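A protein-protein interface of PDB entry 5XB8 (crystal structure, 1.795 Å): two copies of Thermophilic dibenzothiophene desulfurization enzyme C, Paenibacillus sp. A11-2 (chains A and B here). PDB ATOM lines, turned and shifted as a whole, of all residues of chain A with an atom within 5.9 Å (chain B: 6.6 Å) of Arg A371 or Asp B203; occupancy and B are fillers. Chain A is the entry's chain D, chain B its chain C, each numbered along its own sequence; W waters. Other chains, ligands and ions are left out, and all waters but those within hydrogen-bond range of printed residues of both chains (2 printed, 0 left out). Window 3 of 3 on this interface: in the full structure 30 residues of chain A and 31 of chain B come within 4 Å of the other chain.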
ATOM      1  N   ALA A 367     -21.151  19.583   8.590  1.00  0.00           N
ATOM      2  CA  ALA A 367     -21.398  19.688  10.025  1.00  0.00           C
ATOM      3  C   ALA A 367     -22.486  18.728  10.489  1.00  0.00           C
ATOM      4  O   ALA A 367     -22.471  18.299  11.652  1.00  0.00           O
ATOM      5  CB  ALA A 367     -21.769  21.122  10.386  1.00  0.00           C
ATOM      6  N   ALA A 368     -23.443  18.394   9.615  1.00  0.00           N
ATOM      7  CA  ALA A 368     -24.463  17.408   9.920  1.00  0.00           C
ATOM      8  C   ALA A 368     -24.126  16.029   9.375  1.00  0.00           C
ATOM      9  O   ALA A 368     -24.663  15.036   9.867  1.00  0.00           O
ATOM     10  CB  ALA A 368     -25.824  17.836   9.354  1.00  0.00           C
ATOM     11  N   ALA A 369     -23.265  15.944   8.368  1.00  0.00           N
ATOM     12  CA  ALA A 369     -22.975  14.640   7.784  1.00  0.00           C
ATOM     13  C   ALA A 369     -22.141  13.798   8.731  1.00  0.00           C
ATOM     14  O   ALA A 369     -22.215  12.561   8.693  1.00  0.00           O
ATOM     15  CB  ALA A 369     -22.263  14.820   6.444  1.00  0.00           C
ATOM     16  N   SER A 370     -21.368  14.446   9.593  1.00  0.00           N
ATOM     17  CA  SER A 370     -20.533  13.770  10.578  1.00  0.00           C
ATOM     18  C   SER A 370     -21.225  13.864  11.927  1.00  0.00           C
ATOM     19  O   SER A 370     -21.122  14.877  12.622  1.00  0.00           O
ATOM     20  CB  SER A 370     -19.141  14.389  10.622  1.00  0.00           C
ATOM     21  OG  SER A 370     -18.498  14.111  11.862  1.00  0.00           O
ATOM     22  N   ARG A 371     -21.927  12.798  12.303  1.00  0.00           N
ATOM     23  CA  ARG A 371     -22.606  12.788  13.590  1.00  0.00           C
ATOM     24  C   ARG A 371     -21.640  13.102  14.726  1.00  0.00           C
ATOM     25  O   ARG A 371     -22.018  13.774  15.694  1.00  0.00           O
ATOM     26  CB  ARG A 371     -23.276  11.431  13.825  1.00  0.00           C
ATOM     27  CG  ARG A 371     -24.033  11.320  15.156  1.00  0.00           C
ATOM     28  CD  ARG A 371     -24.615   9.919  15.406  1.00  0.00           C
ATOM     29  NE  ARG A 371     -23.586   8.890  15.312  1.00  0.00           N
ATOM     30  CZ  ARG A 371     -22.703   8.621  16.270  1.00  0.00           C
ATOM     31  NH1 ARG A 371     -22.721   9.302  17.412  1.00  0.00           N
ATOM     32  NH2 ARG A 371     -21.795   7.672  16.086  1.00  0.00           N
ATOM     33  N   GLN A 372     -20.383  12.667  14.604  1.00  0.00           N
ATOM     34  CA  GLN A 372     -19.424  12.781  15.701  1.00  0.00           C
ATOM     35  C   GLN A 372     -19.123  14.220  16.076  1.00  0.00           C
ATOM     36  O   GLN A 372     -18.677  14.475  17.202  1.00  0.00           O
ATOM     37  CB  GLN A 372     -18.124  12.061  15.337  1.00  0.00           C
ATOM     38  N   PHE A 373     -19.336  15.166  15.169  1.00  0.00           N
ATOM     39  CA  PHE A 373     -19.116  16.562  15.510  1.00  0.00           C
ATOM     40  C   PHE A 373     -19.991  16.961  16.694  1.00  0.00           C
ATOM     41  O   PHE A 373     -19.558  17.715  17.569  1.00  0.00           O
ATOM     42  CB  PHE A 373     -19.388  17.421  14.279  1.00  0.00           C
ATOM     43  CG  PHE A 373     -19.322  18.894  14.524  1.00  0.00           C
ATOM     44  CD1 PHE A 373     -18.326  19.451  15.315  1.00  0.00           C
ATOM     45  CD2 PHE A 373     -20.237  19.725  13.929  1.00  0.00           C
ATOM     46  CE1 PHE A 373     -18.280  20.800  15.522  1.00  0.00           C
ATOM     47  CE2 PHE A 373     -20.187  21.088  14.120  1.00  0.00           C
ATOM     48  CZ  PHE A 373     -19.218  21.628  14.925  1.00  0.00           C
ATOM     49  N   GLY A 374     -21.209  16.426  16.753  1.00  0.00           N
ATOM     50  CA  GLY A 374     -22.043  16.529  17.935  1.00  0.00           C
ATOM     51  C   GLY A 374     -22.659  17.887  18.195  1.00  0.00           C
ATOM     52  O   GLY A 374     -23.122  18.136  19.307  1.00  0.00           O
ATOM     53  N   PHE A 375     -22.721  18.757  17.189  1.00  0.00           N
ATOM     54  CA  PHE A 375     -23.261  20.095  17.392  1.00  0.00           C
ATOM     55  C   PHE A 375     -24.735  20.078  17.763  1.00  0.00           C
ATOM     56  O   PHE A 375     -25.198  21.026  18.405  1.00  0.00           O
ATOM     57  CB  PHE A 375     -23.052  20.944  16.129  1.00  0.00           C
ATOM     58  CG  PHE A 375     -23.426  22.391  16.305  1.00  0.00           C
ATOM     59  CD1 PHE A 375     -22.543  23.281  16.892  1.00  0.00           C
ATOM     60  CD2 PHE A 375     -24.664  22.858  15.896  1.00  0.00           C
ATOM     61  CE1 PHE A 375     -22.875  24.609  17.061  1.00  0.00           C
ATOM     62  CE2 PHE A 375     -24.999  24.206  16.073  1.00  0.00           C
ATOM     63  CZ  PHE A 375     -24.102  25.069  16.655  1.00  0.00           C
ATOM     64  N   ASP A 376     -25.466  19.022  17.396  1.00  0.00           N
ATOM     65  CA  ASP A 376     -26.900  18.942  17.675  1.00  0.00           C
ATOM     66  C   ASP A 376     -27.185  18.901  19.169  1.00  0.00           C
ATOM     67  O   ASP A 376     -28.337  19.083  19.581  1.00  0.00           O
ATOM     68  CB  ASP A 376     -27.498  17.706  16.995  1.00  0.00           C
ATOM     69  CG  ASP A 376     -26.887  16.411  17.491  1.00  0.00           C
ATOM     70  OD1 ASP A 376     -25.667  16.217  17.290  1.00  0.00           O
ATOM     71  OD2 ASP A 376     -27.618  15.595  18.090  1.00  0.00           O
ATOM     72  N   GLY B 200     -18.545   2.433   3.346  1.00  0.00           N
ATOM     73  CA  GLY B 200     -19.410   2.196   4.500  1.00  0.00           C
ATOM     74  C   GLY B 200     -19.129   3.096   5.687  1.00  0.00           C
ATOM     75  O   GLY B 200     -19.246   2.656   6.838  1.00  0.00           O
ATOM     76  N   ASP B 201     -18.774   4.359   5.436  1.00  0.00           N
ATOM     77  CA  ASP B 201     -18.388   5.286   6.489  1.00  0.00           C
ATOM     78  C   ASP B 201     -19.422   6.388   6.724  1.00  0.00           C
ATOM     79  O   ASP B 201     -19.077   7.466   7.208  1.00  0.00           O
ATOM     80  CB  ASP B 201     -17.033   5.908   6.166  1.00  0.00           C
ATOM     81  CG  ASP B 201     -16.967   6.468   4.744  1.00  0.00           C
ATOM     82  OD1 ASP B 201     -17.974   6.368   4.012  1.00  0.00           O
ATOM     83  OD2 ASP B 201     -15.908   7.000   4.355  1.00  0.00           O
ATOM     84  N   TRP B 202     -20.681   6.141   6.397  1.00  0.00           N
ATOM     85  CA  TRP B 202     -21.733   7.128   6.610  1.00  0.00           C
ATOM     86  C   TRP B 202     -22.240   7.001   8.038  1.00  0.00           C
ATOM     87  O   TRP B 202     -22.758   5.948   8.429  1.00  0.00           O
ATOM     88  CB  TRP B 202     -22.864   6.927   5.614  1.00  0.00           C
ATOM     89  CG  TRP B 202     -24.022   7.896   5.696  1.00  0.00           C
ATOM     90  CD1 TRP B 202     -25.312   7.582   5.988  1.00  0.00           C
ATOM     91  CD2 TRP B 202     -24.009   9.312   5.431  1.00  0.00           C
ATOM     92  NE1 TRP B 202     -26.103   8.696   5.919  1.00  0.00           N
ATOM     93  CE2 TRP B 202     -25.333   9.774   5.589  1.00  0.00           C
ATOM     94  CE3 TRP B 202     -23.017  10.225   5.071  1.00  0.00           C
ATOM     95  CZ2 TRP B 202     -25.688  11.107   5.415  1.00  0.00           C
ATOM     96  CZ3 TRP B 202     -23.368  11.552   4.909  1.00  0.00           C
ATOM     97  CH2 TRP B 202     -24.698  11.978   5.075  1.00  0.00           C
ATOM     98  N   ASP B 203     -22.094   8.073   8.809  1.00  0.00           N
ATOM     99  CA  ASP B 203     -22.532   8.072  10.205  1.00  0.00           C
ATOM    100  C   ASP B 203     -22.961   9.507  10.511  1.00  0.00           C
ATOM    101  O   ASP B 203     -22.150  10.328  10.948  1.00  0.00           O
ATOM    102  CB  ASP B 203     -21.417   7.591  11.120  1.00  0.00           C
ATOM    103  CG  ASP B 203     -21.829   7.566  12.575  1.00  0.00           C
ATOM    104  OD1 ASP B 203     -23.041   7.596  12.870  1.00  0.00           O
ATOM    105  OD2 ASP B 203     -20.929   7.514  13.426  1.00  0.00           O
ATOM    106  N   SER B 204     -24.232   9.793  10.247  1.00  0.00           N
ATOM    107  CA  SER B 204     -24.720  11.157  10.094  1.00  0.00           C
ATOM    108  C   SER B 204     -25.712  11.524  11.190  1.00  0.00           C
ATOM    109  O   SER B 204     -26.229  10.674  11.910  1.00  0.00           O
ATOM    110  CB  SER B 204     -25.382  11.312   8.728  1.00  0.00           C
ATOM    111  OG  SER B 204     -26.455  10.392   8.619  1.00  0.00           O
ATOM    112  N   LEU B 205     -25.967  12.831  11.309  1.00  0.00           N
ATOM    113  CA  LEU B 205     -26.968  13.314  12.258  1.00  0.00           C
ATOM    114  C   LEU B 205     -28.340  12.762  11.911  1.00  0.00           C
ATOM    115  O   LEU B 205     -29.016  12.154  12.754  1.00  0.00           O
ATOM    116  CB  LEU B 205     -26.985  14.838  12.243  1.00  0.00           C
ATOM    117  CG  LEU B 205     -28.090  15.520  13.066  1.00  0.00           C
ATOM    118  CD1 LEU B 205     -27.899  15.242  14.549  1.00  0.00           C
ATOM    119  CD2 LEU B 205     -28.083  16.997  12.804  1.00  0.00           C
ATOM    120  N   GLY B 206     -28.753  12.968  10.659  1.00  0.00           N
ATOM    121  CA  GLY B 206     -30.004  12.469  10.135  1.00  0.00           C
ATOM    122  C   GLY B 206     -29.762  11.897   8.749  1.00  0.00           C
ATOM    123  O   GLY B 206     -28.622  11.804   8.300  1.00  0.00           O
ATOM    124  N   ARG B 208     -29.972   8.859   8.172  1.00  0.00           N
ATOM    125  CA  ARG B 208     -28.930   7.927   8.614  1.00  0.00           C
ATOM    126  C   ARG B 208     -28.879   6.625   7.816  1.00  0.00           C
ATOM    127  O   ARG B 208     -27.870   5.908   7.900  1.00  0.00           O
ATOM    128  CB  ARG B 208     -29.094   7.610  10.109  1.00  0.00           C
ATOM    129  CG  ARG B 208     -28.666   8.777  10.974  1.00  0.00           C
ATOM    130  CD  ARG B 208     -28.751   8.485  12.481  1.00  0.00           C
ATOM    131  NE  ARG B 208     -28.120   7.226  12.862  1.00  0.00           N
ATOM    132  CZ  ARG B 208     -26.810   7.018  12.981  1.00  0.00           C
ATOM    133  NH1 ARG B 208     -25.922   7.977  12.733  1.00  0.00           N
ATOM    134  NH2 ARG B 208     -26.380   5.812  13.341  1.00  0.00           N
ATOM    135  N   GLY B 213     -21.921   7.695   2.219  1.00  0.00           N
ATOM    136  CA  GLY B 213     -20.511   7.788   2.522  1.00  0.00           C
ATOM    137  C   GLY B 213     -19.643   7.794   1.275  1.00  0.00           C
ATOM    138  O   GLY B 213     -20.092   8.091   0.166  1.00  0.00           O
HETATM  139  O   HOH W   1     -20.714  10.470   7.948  1.00  0.00           O
HETATM  140  O   HOH W   2     -19.651  10.582  12.763  1.00  0.00           O
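Water W1 bridges the backbone carbonyl oxygen (O) of Ala A369 (2.7 Å) and the backbone NH (N) of Asp B203 (2.9 Å).
Water W2 lies within hydrogen-bond range of N of Gln A372 (2.9 Å), O of Asp B203 (3.1 Å) and N of Arg A371 (3.2 Å).
NH1 of Arg B208 lies within salt-bridge range of OD1 of Asp B203 (2.9 Å).
O of Gly B206 lies within hydrogen-bond range of OG of Ser B204 (2.6 Å).
NE1 of Trp B202 is in hydrogen-bond range of OG of Ser B204 (3.2 Å).
The backbone carbonyl oxygen (O) of Ser B204 lies within hydrogen-bond range of the guanidinium group (NH1) of Arg B208 (2.8 Å).
Along chain A the printed residues that touch a printed residue of chain B span positions 368 to 376.
Printed residues of chain B that touch a printed residue of chain A: Trp B202, Asp B203, Ser B204, Leu B205 and Arg B208.
Hydrophobic or aromatic side chains of chain B that line the printed part of chain A: Trp B202 and Leu B205.
Among the printed residues, 11 pairs touch across the chains.
Among the printed residues, Asp or Glu carboxylates within 4 Å of a Lys or Arg side-chain nitrogen of the other chain: Arg A371 with Asp B203.
NH2 of Arg A371 lies within salt-bridge range of OD2 of Asp B203, 2.8 Å away.
The backbone carbonyl oxygen (O) of Asp B203 sits close to the backbone carbonyl oxygen (O) of Ala A369.
The backbone NH (N) of Leu B205 lies within hydrogen-bond range of the backbone carbonyl oxygen (O) of Ala A368 (2.9 Å).
Among the printed residues, merely in contact across the chains: Ala A369 with Ser B204, Asp A376 with Leu B205, Arg A371 with Arg B208, Arg A371 with Ser B204, Ala A369 with Trp B202, Ser A370 with Asp B203, Ala A368 with Ser B204 and Arg A371 with Leu B205.
Printed residues of chain B within 4 Å of Ala A369: Trp B202 (3.8 Å), Asp B203 (3.2 Å) and Ser B204 (3.2 Å).
Arg A371 touches four residues of chain B.
Gln A372 touches none of the printed residues of chain B.
Printed residues of chain B within 4 Å of Asp A376: Leu B205.
Of the printed residues of chain A, Trp B202 touches Ala A369.
Asp B203 touches just these residues of chain A: Ala A369 (3.2 Å), Ser A370 (3.8 Å) and Arg A371 (2.8 Å).
Gly B206 touches none of the printed residues of chain A.
Printed residues of chain A within 4 Å of Arg B208: Arg A371.
No position is printed for both chains.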
